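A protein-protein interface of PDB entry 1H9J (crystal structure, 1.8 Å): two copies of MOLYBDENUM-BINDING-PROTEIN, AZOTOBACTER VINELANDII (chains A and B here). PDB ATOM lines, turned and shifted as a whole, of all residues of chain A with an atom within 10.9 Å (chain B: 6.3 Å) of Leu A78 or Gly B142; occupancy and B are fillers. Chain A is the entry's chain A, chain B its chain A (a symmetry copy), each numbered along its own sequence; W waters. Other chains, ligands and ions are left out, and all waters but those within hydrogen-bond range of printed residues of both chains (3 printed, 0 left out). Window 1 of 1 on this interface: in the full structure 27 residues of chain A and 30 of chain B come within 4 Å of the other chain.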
ATOM      1  N   VAL A  67      18.282  -3.210  10.395  1.00  0.00           N
ATOM      2  CA  VAL A  67      17.530  -1.978  10.605  1.00  0.00           C
ATOM      3  C   VAL A  67      18.443  -0.774  10.752  1.00  0.00           C
ATOM      4  O   VAL A  67      19.284  -0.766  11.678  1.00  0.00           O
ATOM      5  CB  VAL A  67      16.680  -2.094  11.914  1.00  0.00           C
ATOM      6  CG1 VAL A  67      15.821  -0.844  12.148  1.00  0.00           C
ATOM      7  CG2 VAL A  67      15.860  -3.383  11.809  1.00  0.00           C
ATOM      8  N   LEU A  68      18.272   0.189   9.849  1.00  0.00           N
ATOM      9  CA  LEU A  68      19.092   1.416   9.948  1.00  0.00           C
ATOM     10  C   LEU A  68      18.284   2.408  10.780  1.00  0.00           C
ATOM     11  O   LEU A  68      17.072   2.228  10.973  1.00  0.00           O
ATOM     12  CB  LEU A  68      19.281   2.058   8.578  1.00  0.00           C
ATOM     13  CG  LEU A  68      20.365   1.467   7.678  1.00  0.00           C
ATOM     14  CD1 LEU A  68      19.859   0.208   6.997  1.00  0.00           C
ATOM     15  CD2 LEU A  68      20.830   2.491   6.635  1.00  0.00           C
ATOM     16  N   LEU A  69      18.980   3.311  11.473  1.00  0.00           N
ATOM     17  CA  LEU A  69      18.239   4.337  12.221  1.00  0.00           C
ATOM     18  C   LEU A  69      18.438   5.704  11.583  1.00  0.00           C
ATOM     19  O   LEU A  69      19.613   5.977  11.270  1.00  0.00           O
ATOM     20  CB  LEU A  69      18.730   4.404  13.649  1.00  0.00           C
ATOM     21  CG  LEU A  69      18.367   3.140  14.476  1.00  0.00           C
ATOM     22  CD1 LEU A  69      19.058   3.263  15.834  1.00  0.00           C
ATOM     23  CD2 LEU A  69      16.861   3.088  14.608  1.00  0.00           C
ATOM     24  N   MET A  70      17.464   6.597  11.447  1.00  0.00           N
ATOM     25  CA  MET A  70      17.681   7.915  10.853  1.00  0.00           C
ATOM     26  C   MET A  70      17.035   8.949  11.782  1.00  0.00           C
ATOM     27  O   MET A  70      15.943   8.666  12.271  1.00  0.00           O
ATOM     28  CB  MET A  70      17.035   7.985   9.462  1.00  0.00           C
ATOM     29  CG  MET A  70      17.024   9.331   8.779  1.00  0.00           C
ATOM     30  SD  MET A  70      16.556   9.178   7.055  1.00  0.00           S
ATOM     31  CE  MET A  70      14.833   8.761   7.218  1.00  0.00           C
ATOM     32  N   THR A  71      17.661  10.072  12.029  1.00  0.00           N
ATOM     33  CA  THR A  71      17.076  11.139  12.839  1.00  0.00           C
ATOM     34  C   THR A  71      16.704  12.346  11.978  1.00  0.00           C
ATOM     35  O   THR A  71      16.106  13.238  12.591  1.00  0.00           O
ATOM     36  CB  THR A  71      17.974  11.676  13.955  1.00  0.00           C
ATOM     37  OG1 THR A  71      19.294  11.971  13.448  1.00  0.00           O
ATOM     38  CG2 THR A  71      18.060  10.603  15.043  1.00  0.00           C
ATOM     39  N   ASP A  72      17.349  12.648  10.901  1.00  0.00           N
ATOM     40  CA  ASP A  72      17.073  13.864  10.117  1.00  0.00           C
ATOM     41  C   ASP A  72      17.234  13.452   8.663  1.00  0.00           C
ATOM     42  O   ASP A  72      18.342  13.096   8.252  1.00  0.00           O
ATOM     43  CB  ASP A  72      17.951  15.051  10.490  1.00  0.00           C
ATOM     44  CG  ASP A  72      17.476  16.370   9.902  1.00  0.00           C
ATOM     45  OD1 ASP A  72      18.113  17.420  10.146  1.00  0.00           O
ATOM     46  OD2 ASP A  72      16.447  16.375   9.191  1.00  0.00           O
ATOM     47  N   SER A  73      16.104  13.411   7.966  1.00  0.00           N
ATOM     48  CA  SER A  73      16.113  13.028   6.562  1.00  0.00           C
ATOM     49  C   SER A  73      16.662  14.167   5.711  1.00  0.00           C
ATOM     50  O   SER A  73      17.141  14.006   4.600  1.00  0.00           O
ATOM     51  CB  SER A  73      14.700  12.653   6.089  1.00  0.00           C
ATOM     52  OG  SER A  73      13.831  13.784   6.169  1.00  0.00           O
ATOM     53  N   SER A  74      16.505  15.378   6.265  1.00  0.00           N
ATOM     54  CA  SER A  74      16.931  16.613   5.626  1.00  0.00           C
ATOM     55  C   SER A  74      16.296  16.751   4.249  1.00  0.00           C
ATOM     56  O   SER A  74      17.057  16.992   3.294  1.00  0.00           O
ATOM     57  CB  SER A  74      18.436  16.618   5.505  1.00  0.00           C
ATOM     58  OG  SER A  74      19.031  17.867   5.218  1.00  0.00           O
ATOM     59  N   GLY A  75      15.030  16.361   4.135  1.00  0.00           N
ATOM     60  CA  GLY A  75      14.368  16.420   2.831  1.00  0.00           C
ATOM     61  C   GLY A  75      14.563  15.241   1.907  1.00  0.00           C
ATOM     62  O   GLY A  75      13.836  15.065   0.911  1.00  0.00           O
ATOM     63  N   TYR A  76      15.549  14.386   2.162  1.00  0.00           N
ATOM     64  CA  TYR A  76      15.780  13.240   1.294  1.00  0.00           C
ATOM     65  C   TYR A  76      14.644  12.219   1.365  1.00  0.00           C
ATOM     66  O   TYR A  76      14.027  11.988   2.404  1.00  0.00           O
ATOM     67  CB  TYR A  76      17.086  12.519   1.616  1.00  0.00           C
ATOM     68  CG  TYR A  76      18.315  13.240   1.093  1.00  0.00           C
ATOM     69  CD1 TYR A  76      18.877  14.284   1.826  1.00  0.00           C
ATOM     70  CD2 TYR A  76      18.930  12.873  -0.071  1.00  0.00           C
ATOM     71  CE1 TYR A  76      20.008  14.924   1.361  1.00  0.00           C
ATOM     72  CE2 TYR A  76      20.028  13.530  -0.597  1.00  0.00           C
ATOM     73  CZ  TYR A  76      20.575  14.566   0.162  1.00  0.00           C
ATOM     74  OH  TYR A  76      21.705  15.216  -0.292  1.00  0.00           O
ATOM     75  N   ARG A  77      14.436  11.585   0.214  1.00  0.00           N
ATOM     76  CA  ARG A  77      13.462  10.511   0.065  1.00  0.00           C
ATOM     77  C   ARG A  77      14.308   9.263  -0.189  1.00  0.00           C
ATOM     78  O   ARG A  77      15.236   9.392  -1.004  1.00  0.00           O
ATOM     79  CB  ARG A  77      12.536  10.776  -1.127  1.00  0.00           C
ATOM     80  CG  ARG A  77      11.620  11.988  -1.037  1.00  0.00           C
ATOM     81  CD  ARG A  77      10.843  12.224  -2.348  1.00  0.00           C
ATOM     82  NE  ARG A  77      11.685  12.695  -3.441  1.00  0.00           N
ATOM     83  CZ  ARG A  77      11.393  12.661  -4.741  1.00  0.00           C
ATOM     84  NH1 ARG A  77      10.238  12.151  -5.168  1.00  0.00           N
ATOM     85  NH2 ARG A  77      12.231  13.109  -5.670  1.00  0.00           N
ATOM     86  N   LEU A  78      14.024   8.140   0.457  1.00  0.00           N
ATOM     87  CA  LEU A  78      14.910   6.984   0.242  1.00  0.00           C
ATOM     88  C   LEU A  78      14.237   5.860  -0.544  1.00  0.00           C
ATOM     89  O   LEU A  78      13.007   5.804  -0.605  1.00  0.00           O
ATOM     90  CB  LEU A  78      15.360   6.376   1.592  1.00  0.00           C
ATOM     91  CG  LEU A  78      15.930   7.360   2.615  1.00  0.00           C
ATOM     92  CD1 LEU A  78      16.095   6.749   4.016  1.00  0.00           C
ATOM     93  CD2 LEU A  78      17.222   7.996   2.121  1.00  0.00           C
ATOM     94  N   SER A  79      15.041   4.941  -1.094  1.00  0.00           N
ATOM     95  CA  SER A  79      14.498   3.813  -1.832  1.00  0.00           C
ATOM     96  C   SER A  79      13.967   2.708  -0.912  1.00  0.00           C
ATOM     97  O   SER A  79      13.111   1.949  -1.394  1.00  0.00           O
ATOM     98  CB  SER A  79      15.553   3.172  -2.733  1.00  0.00           C
ATOM     99  OG  SER A  79      16.656   2.719  -1.979  1.00  0.00           O
ATOM    100  N   ALA A  80      14.471   2.607   0.327  1.00  0.00           N
ATOM    101  CA  ALA A  80      13.830   1.620   1.219  1.00  0.00           C
ATOM    102  C   ALA A  80      12.360   1.892   1.490  1.00  0.00           C
ATOM    103  O   ALA A  80      12.002   3.025   1.813  1.00  0.00           O
ATOM    104  CB  ALA A  80      14.520   1.748   2.609  1.00  0.00           C
ATOM    105  N   ARG A  81      11.539   0.860   1.440  1.00  0.00           N
ATOM    106  CA  ARG A  81      10.095   1.034   1.580  1.00  0.00           C
ATOM    107  C   ARG A  81       9.589   1.351   2.979  1.00  0.00           C
ATOM    108  O   ARG A  81       8.563   2.046   3.076  1.00  0.00           O
ATOM    109  CB  ARG A  81       9.443  -0.279   1.104  1.00  0.00           C
ATOM    110  N   ASN A  82      10.243   0.895   4.046  1.00  0.00           N
ATOM    111  CA  ASN A  82       9.784   1.032   5.403  1.00  0.00           C
ATOM    112  C   ASN A  82      10.581   2.083   6.193  1.00  0.00           C
ATOM    113  O   ASN A  82      11.789   1.915   6.279  1.00  0.00           O
ATOM    114  CB  ASN A  82       9.934  -0.295   6.199  1.00  0.00           C
ATOM    115  CG  ASN A  82       9.177  -1.397   5.494  1.00  0.00           C
ATOM    116  OD1 ASN A  82       7.928  -1.232   5.391  1.00  0.00           O
ATOM    117  ND2 ASN A  82       9.813  -2.439   4.940  1.00  0.00           N
ATOM    118  N   ILE A  83       9.898   3.151   6.568  1.00  0.00           N
ATOM    119  CA  ILE A  83      10.425   4.253   7.363  1.00  0.00           C
ATOM    120  C   ILE A  83       9.476   4.420   8.551  1.00  0.00           C
ATOM    121  O   ILE A  83       8.444   5.097   8.407  1.00  0.00           O
ATOM    122  CB  ILE A  83      10.637   5.562   6.596  1.00  0.00           C
ATOM    123  CG1 ILE A  83      11.613   5.320   5.437  1.00  0.00           C
ATOM    124  CG2 ILE A  83      11.222   6.639   7.517  1.00  0.00           C
ATOM    125  CD1 ILE A  83      11.742   6.482   4.472  1.00  0.00           C
ATOM    126  N   LEU A  84       9.823   3.852   9.713  1.00  0.00           N
ATOM    127  CA  LEU A  84       8.891   3.788  10.844  1.00  0.00           C
ATOM    128  C   LEU A  84       9.348   4.753  11.928  1.00  0.00           C
ATOM    129  O   LEU A  84      10.432   4.519  12.459  1.00  0.00           O
ATOM    130  CB  LEU A  84       8.779   2.393  11.453  1.00  0.00           C
ATOM    131  CG  LEU A  84       8.563   1.248  10.443  1.00  0.00           C
ATOM    132  CD1 LEU A  84       8.376  -0.076  11.163  1.00  0.00           C
ATOM    133  CD2 LEU A  84       7.332   1.501   9.578  1.00  0.00           C
ATOM    134  N   THR A  85       8.459   5.727  12.203  1.00  0.00           N
ATOM    135  CA  THR A  85       8.941   6.711  13.196  1.00  0.00           C
ATOM    136  C   THR A  85       8.606   6.366  14.617  1.00  0.00           C
ATOM    137  O   THR A  85       7.524   5.823  14.902  1.00  0.00           O
ATOM    138  CB  THR A  85       8.348   8.083  12.834  1.00  0.00           C
ATOM    139  OG1 THR A  85       6.914   7.953  12.826  1.00  0.00           O
ATOM    140  CG2 THR A  85       8.896   8.501  11.486  1.00  0.00           C
ATOM    141  N   ALA A 130      13.367   9.077  16.332  1.00  0.00           N
ATOM    142  CA  ALA A 130      14.185   8.529  15.238  1.00  0.00           C
ATOM    143  C   ALA A 130      13.351   7.554  14.426  1.00  0.00           C
ATOM    144  O   ALA A 130      12.293   7.159  14.892  1.00  0.00           O
ATOM    145  CB  ALA A 130      15.362   7.750  15.821  1.00  0.00           C
ATOM    146  N   SER A 131      13.773   7.361  13.178  1.00  0.00           N
ATOM    147  CA  SER A 131      13.015   6.418  12.369  1.00  0.00           C
ATOM    148  C   SER A 131      13.810   5.139  12.135  1.00  0.00           C
ATOM    149  O   SER A 131      15.004   5.246  11.813  1.00  0.00           O
ATOM    150  CB  SER A 131      12.799   7.029  10.970  1.00  0.00           C
ATOM    151  OG  SER A 131      12.053   8.232  11.142  1.00  0.00           O
ATOM    152  N   ALA A 132      13.159   4.013  12.047  1.00  0.00           N
ATOM    153  CA  ALA A 132      13.772   2.745  11.701  1.00  0.00           C
ATOM    154  C   ALA A 132      13.599   2.660  10.178  1.00  0.00           C
ATOM    155  O   ALA A 132      12.444   2.645   9.718  1.00  0.00           O
ATOM    156  CB  ALA A 132      13.054   1.595  12.367  1.00  0.00           C
ATOM    157  N   VAL A 133      14.658   2.355   9.450  1.00  0.00           N
ATOM    158  CA  VAL A 133      14.577   2.266   7.985  1.00  0.00           C
ATOM    159  C   VAL A 133      14.899   0.806   7.647  1.00  0.00           C
ATOM    160  O   VAL A 133      15.960   0.307   8.056  1.00  0.00           O
ATOM    161  CB  VAL A 133      15.610   3.166   7.295  1.00  0.00           C
ATOM    162  CG1 VAL A 133      15.603   3.056   5.764  1.00  0.00           C
ATOM    163  CG2 VAL A 133      15.319   4.642   7.677  1.00  0.00           C
ATOM    164  N   ILE A 134      13.931   0.139   7.032  1.00  0.00           N
ATOM    165  CA  ILE A 134      14.093  -1.259   6.670  1.00  0.00           C
ATOM    166  C   ILE A 134      13.691  -1.521   5.227  1.00  0.00           C
ATOM    167  O   ILE A 134      12.631  -1.094   4.787  1.00  0.00           O
ATOM    168  CB  ILE A 134      13.224  -2.197   7.544  1.00  0.00           C
ATOM    169  CG1 ILE A 134      13.423  -1.896   9.042  1.00  0.00           C
ATOM    170  CG2 ILE A 134      13.582  -3.646   7.225  1.00  0.00           C
ATOM    171  CD1 ILE A 134      12.346  -2.526   9.911  1.00  0.00           C
ATOM    172  N   LYS A 135      14.603  -2.113   4.426  1.00  0.00           N
ATOM    173  CA  LYS A 135      14.242  -2.511   3.078  1.00  0.00           C
ATOM    174  C   LYS A 135      13.180  -3.599   3.133  1.00  0.00           C
ATOM    175  O   LYS A 135      13.388  -4.541   3.899  1.00  0.00           O
ATOM    176  CB  LYS A 135      15.468  -3.202   2.428  1.00  0.00           C
ATOM    177  CG  LYS A 135      16.461  -2.169   1.863  1.00  0.00           C
ATOM    178  CD  LYS A 135      17.482  -2.878   0.974  1.00  0.00           C
ATOM    179  CE  LYS A 135      16.736  -3.140  -0.357  1.00  0.00           C
ATOM    180  NZ  LYS A 135      17.755  -3.352  -1.416  1.00  0.00           N
ATOM    181  N   ALA A 136      12.189  -3.531   2.216  1.00  0.00           N
ATOM    182  CA  ALA A 136      11.154  -4.602   2.316  1.00  0.00           C
ATOM    183  C   ALA A 136      11.722  -5.962   1.973  1.00  0.00           C
ATOM    184  O   ALA A 136      11.302  -6.999   2.488  1.00  0.00           O
ATOM    185  CB  ALA A 136       9.990  -4.258   1.387  1.00  0.00           C
ATOM    186  N   MET B   4      21.704  14.843   5.990  1.00  0.00           N
ATOM    187  CA  MET B   4      20.976  13.578   6.433  1.00  0.00           C
ATOM    188  C   MET B   4      21.682  12.813   7.542  1.00  0.00           C
ATOM    189  O   MET B   4      22.891  12.651   7.370  1.00  0.00           O
ATOM    190  CB  MET B   4      20.703  12.765   5.151  1.00  0.00           C
ATOM    191  CG  MET B   4      20.575  11.275   5.491  1.00  0.00           C
ATOM    192  SD  MET B   4      20.214  10.273   4.058  1.00  0.00           S
ATOM    193  CE  MET B   4      20.780   8.667   4.542  1.00  0.00           C
ATOM    194  N   ILE B   6      22.050   9.609   9.464  1.00  0.00           N
ATOM    195  CA  ILE B   6      21.655   8.183   9.414  1.00  0.00           C
ATOM    196  C   ILE B   6      22.762   7.322   9.992  1.00  0.00           C
ATOM    197  O   ILE B   6      23.950   7.671   9.959  1.00  0.00           O
ATOM    198  CB  ILE B   6      21.290   7.738   7.995  1.00  0.00           C
ATOM    199  CG1 ILE B   6      20.552   6.419   7.989  1.00  0.00           C
ATOM    200  CG2 ILE B   6      22.524   7.711   7.081  1.00  0.00           C
ATOM    201  CD1 ILE B   6      19.674   6.244   6.730  1.00  0.00           C
ATOM    202  N   SER B  46      10.714   2.441  -7.221  1.00  0.00           N
ATOM    203  CA  SER B  46      11.546   3.478  -6.638  1.00  0.00           C
ATOM    204  C   SER B  46      12.237   4.318  -7.713  1.00  0.00           C
ATOM    205  O   SER B  46      12.364   5.539  -7.500  1.00  0.00           O
ATOM    206  CB  SER B  46      12.627   2.883  -5.723  1.00  0.00           C
ATOM    207  OG  SER B  46      11.975   2.406  -4.538  1.00  0.00           O
ATOM    208  N   SER B  49       9.538   6.724  -8.808  1.00  0.00           N
ATOM    209  CA  SER B  49       9.090   7.642  -7.760  1.00  0.00           C
ATOM    210  C   SER B  49      10.141   8.654  -7.341  1.00  0.00           C
ATOM    211  O   SER B  49       9.822   9.794  -6.948  1.00  0.00           O
ATOM    212  CB  SER B  49       8.601   6.859  -6.531  1.00  0.00           C
ATOM    213  OG  SER B  49       9.709   6.451  -5.746  1.00  0.00           O
ATOM    214  N   LEU B  50      11.392   8.220  -7.204  1.00  0.00           N
ATOM    215  CA  LEU B  50      12.519   9.080  -6.888  1.00  0.00           C
ATOM    216  C   LEU B  50      12.942   9.951  -8.086  1.00  0.00           C
ATOM    217  O   LEU B  50      13.904  10.770  -7.923  1.00  0.00           O
ATOM    218  CB  LEU B  50      13.733   8.285  -6.402  1.00  0.00           C
ATOM    219  CG  LEU B  50      13.591   7.315  -5.201  1.00  0.00           C
ATOM    220  CD1 LEU B  50      14.882   6.637  -4.846  1.00  0.00           C
ATOM    221  CD2 LEU B  50      13.035   8.087  -4.002  1.00  0.00           C
ATOM    222  N   GLU B  57      21.908  14.036  -8.982  1.00  0.00           N
ATOM    223  CA  GLU B  57      22.686  13.752  -7.783  1.00  0.00           C
ATOM    224  C   GLU B  57      21.900  12.848  -6.843  1.00  0.00           C
ATOM    225  O   GLU B  57      20.666  12.906  -6.852  1.00  0.00           O
ATOM    226  CB  GLU B  57      23.039  14.995  -6.950  1.00  0.00           C
ATOM    227  CG  GLU B  57      23.696  16.050  -7.822  1.00  0.00           C
ATOM    228  CD  GLU B  57      25.074  15.672  -8.313  1.00  0.00           C
ATOM    229  OE1 GLU B  57      25.530  14.519  -8.199  1.00  0.00           O
ATOM    230  OE2 GLU B  57      25.754  16.583  -8.845  1.00  0.00           O
ATOM    231  N   VAL B  58      22.631  11.903  -6.245  1.00  0.00           N
ATOM    232  CA  VAL B  58      22.022  10.966  -5.296  1.00  0.00           C
ATOM    233  C   VAL B  58      22.977  10.747  -4.094  1.00  0.00           C
ATOM    234  O   VAL B  58      24.181  11.030  -4.083  1.00  0.00           O
ATOM    235  CB  VAL B  58      21.723   9.592  -5.897  1.00  0.00           C
ATOM    236  CG1 VAL B  58      20.694   9.631  -7.034  1.00  0.00           C
ATOM    237  CG2 VAL B  58      23.019   8.951  -6.395  1.00  0.00           C
ATOM    238  N   VAL B  59      22.418  10.140  -3.040  1.00  0.00           N
ATOM    239  CA  VAL B  59      23.258   9.659  -1.938  1.00  0.00           C
ATOM    240  C   VAL B  59      23.155   8.127  -1.918  1.00  0.00           C
ATOM    241  O   VAL B  59      22.091   7.665  -2.294  1.00  0.00           O
ATOM    242  CB  VAL B  59      22.885  10.263  -0.580  1.00  0.00           C
ATOM    243  CG1 VAL B  59      22.992  11.796  -0.663  1.00  0.00           C
ATOM    244  CG2 VAL B  59      21.512   9.863  -0.069  1.00  0.00           C
ATOM    245  N   ALA B  60      24.267   7.425  -1.672  1.00  0.00           N
ATOM    246  CA  ALA B  60      24.190   5.945  -1.618  1.00  0.00           C
ATOM    247  C   ALA B  60      24.549   5.539  -0.151  1.00  0.00           C
ATOM    248  O   ALA B  60      25.486   6.149   0.362  1.00  0.00           O
ATOM    249  CB  ALA B  60      25.144   5.308  -2.599  1.00  0.00           C
ATOM    250  N   VAL B  61      23.706   4.686   0.443  1.00  0.00           N
ATOM    251  CA  VAL B  61      23.858   4.383   1.870  1.00  0.00           C
ATOM    252  C   VAL B  61      24.075   2.892   2.092  1.00  0.00           C
ATOM    253  O   VAL B  61      23.373   2.054   1.510  1.00  0.00           O
ATOM    254  CB  VAL B  61      22.560   4.784   2.617  1.00  0.00           C
ATOM    255  CG1 VAL B  61      22.626   4.339   4.081  1.00  0.00           C
ATOM    256  CG2 VAL B  61      22.329   6.309   2.552  1.00  0.00           C
ATOM    257  N   ILE B 140      21.193   1.319  -0.494  1.00  0.00           N
ATOM    258  CA  ILE B 140      19.987   2.107  -0.418  1.00  0.00           C
ATOM    259  C   ILE B 140      20.281   3.488  -1.020  1.00  0.00           C
ATOM    260  O   ILE B 140      21.340   4.042  -0.739  1.00  0.00           O
ATOM    261  CB  ILE B 140      19.540   2.265   1.051  1.00  0.00           C
ATOM    262  CG1 ILE B 140      18.890   0.940   1.522  1.00  0.00           C
ATOM    263  CG2 ILE B 140      18.445   3.310   1.251  1.00  0.00           C
ATOM    264  CD1 ILE B 140      18.852   0.819   3.076  1.00  0.00           C
ATOM    265  N   LEU B 141      19.394   3.993  -1.854  1.00  0.00           N
ATOM    266  CA  LEU B 141      19.580   5.315  -2.442  1.00  0.00           C
ATOM    267  C   LEU B 141      18.661   6.350  -1.817  1.00  0.00           C
ATOM    268  O   LEU B 141      17.553   6.102  -1.335  1.00  0.00           O
ATOM    269  CB  LEU B 141      19.216   5.261  -3.958  1.00  0.00           C
ATOM    270  CG  LEU B 141      20.115   4.425  -4.851  1.00  0.00           C
ATOM    271  CD1 LEU B 141      19.577   4.408  -6.290  1.00  0.00           C
ATOM    272  CD2 LEU B 141      21.559   4.914  -4.772  1.00  0.00           C
ATOM    273  N   GLY B 142      19.178   7.589  -1.862  1.00  0.00           N
ATOM    274  CA  GLY B 142      18.469   8.744  -1.366  1.00  0.00           C
ATOM    275  C   GLY B 142      18.446   9.833  -2.467  1.00  0.00           C
ATOM    276  O   GLY B 142      19.543   9.990  -3.027  1.00  0.00           O
ATOM    277  N   VAL B 143      17.390  10.609  -2.608  1.00  0.00           N
ATOM    278  CA  VAL B 143      17.453  11.697  -3.585  1.00  0.00           C
ATOM    279  C   VAL B 143      16.937  12.944  -2.847  1.00  0.00           C
ATOM    280  O   VAL B 143      16.026  12.817  -2.010  1.00  0.00           O
ATOM    281  CB  VAL B 143      16.648  11.457  -4.860  1.00  0.00           C
ATOM    282  CG1 VAL B 143      17.097  10.263  -5.694  1.00  0.00           C
ATOM    283  CG2 VAL B 143      15.164  11.286  -4.541  1.00  0.00           C
ATOM    284  N   PRO B 144      17.632  14.056  -3.075  1.00  0.00           N
ATOM    285  CA  PRO B 144      17.262  15.306  -2.439  1.00  0.00           C
ATOM    286  C   PRO B 144      15.870  15.695  -2.906  1.00  0.00           C
ATOM    287  O   PRO B 144      15.482  15.345  -4.019  1.00  0.00           O
ATOM    288  CB  PRO B 144      18.351  16.280  -2.860  1.00  0.00           C
ATOM    289  CG  PRO B 144      19.016  15.693  -4.049  1.00  0.00           C
ATOM    290  CD  PRO B 144      18.772  14.208  -4.007  1.00  0.00           C
HETATM  291  O   HOH W   1      13.640   0.146  -3.975  1.00  0.00           O
HETATM  292  O   HOH W   2      10.777   1.060  -1.974  1.00  0.00           O
HETATM  293  O   HOH W   3      10.942   4.613  -3.098  1.00  0.00           O
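The backbone carbonyl oxygen of Ser B49 sits at hydrogen-bond distance from the guanidinium group of Arg A77.
N of Val B143 is in hydrogen-bond range of O of Arg A77 (2.9 Å).
O of Ser A79 lies within hydrogen-bond range of OG of Ser B46 (3.4 Å).
N of Ser A79 is in hydrogen-bond range of O of Leu B141, 2.8 Å away.
The backbone carbonyl oxygen (O) of Leu A68 is in hydrogen-bond range of the backbone NH (N) of Val A133, 2.9 Å away.
The side-chain carboxylate of Asp A72 is in hydrogen-bond range of the backbone NH of Ser A74 (3.1 Å).
OG of Ser A73 lies close to N of Gly A75 (3.5 Å).
The backbone carbonyl oxygen (O) of Ser B46 sits at hydrogen-bond distance from the side-chain hydroxyl (OG) of Ser B49.
N of Val B59 is in hydrogen-bond range of O of Gly B142, 2.9 Å away.
The backbone NH (N) of Val B61 sits at hydrogen-bond distance from the backbone carbonyl oxygen (O) of Ile B140 (2.7 Å).
O of Leu A69 touches CG1 of Ile B6, 3.4 Å away.
Met B4 touches Asp A72.
Met B4 touches Ser A74.
Tyr A76 touches Val B59 (CE2 to CG1, 3.4 Å).
Tyr A76 touches Gly B142.
Tyr A76 touches Val B143 (CA to O, 3.3 Å).
Arg A77 touches Gly B142 (O to CA, 3.3 Å).
CA of Leu A78 touches O of Leu B141, 3.2 Å away.
Leu A78 touches Gly B142 (CD2 to CA, 3.8 Å).
Lys A135 touches Ile B140 (CG to CG1, 3.96 Å).
Leu A78 touches just these residues of chain B: Leu B141 (3.2 Å) and Gly B142 (3.8 Å).
Gly B142 touches three residues of chain A.
No residue of chain A comes within 4 Å of Val B58.
Val B59 touches just one residue of chain A: Tyr A76.
Ala B60 touches none of the printed residues of chain A.
Of chain A, only Ser A79 (3.7 Å) and Lys A135 (3.96 Å) come within 4 Å of Ile B140.
Leu B141 touches just these residues of chain A: Leu A78 and Ser A79.
Of the printed residues of chain B, Leu A69 touches Ile B6.
Of the printed residues of chain A, Ser B46 touches Ser A79 (3.4 Å).
Of the printed residues of chain A, Leu B50 touches Arg A77.
Printed residues of chain B within 4 Å of Leu A68: Ile B6 and Val B61.
Leu A84 touches none of the printed residues of chain B.
The nearest residue of chain B that does not touch Leu A78 is Leu B50 (4.1 Å).
The nearest printed residue of chain B that does not touch Ser A79 is Leu B50 (4.1 Å).
Of the 15 printed residues of chain B, 12 touch a printed residue of chain A.
Printed residues of chain B that touch a printed residue of chain A: Met B4, Ile B6, Ser B46, Ser B49, Leu B50, Val B59, Val B61, Ile B140, Leu B141, Gly B142, Val B143 and Pro B144.
Hydrophobic or aromatic side chains of chain B that line the printed part of chain A: Met B4, Ile B6, Leu B50, Val B59, Val B61, Ile B140, Val B143 and Pro B144.
Of the 26 printed residues of chain A, 10 touch a printed residue of chain B.
Printed residues of chain A that touch a printed residue of chain B: Leu A68, Leu A69, Asp A72, Ser A73, Ser A74, Tyr A76, Arg A77, Leu A78, Ser A79 and Lys A135.
Hydrophobic or aromatic side chains of chain A that line the printed part of chain B: Leu A68, Tyr A76 and Leu A78.
Among the printed residues, 20 pairs touch across the chains.
Among the printed residues, no Asp or Glu carboxylate lies within 4 Å of a Lys or Arg side-chain nitrogen of the other chain.
No position is printed for both chains.
Of the 20 pairs that touch across the chains among the printed residues, none has its exchanged pair printed and touching as well.
Water W2 lies within hydrogen-bond range of O of Ser A79 and OG of Ser B46.
Water W3 lies within hydrogen-bond range of OG of Ser B46 (2.8 Å), O of Leu A78 (3.4 Å) and OG of Ser B49 (3.5 Å).
Water W1 bridges OG of Ser B46 (2.9 Å) and O of Ser A79 (3.2 Å).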
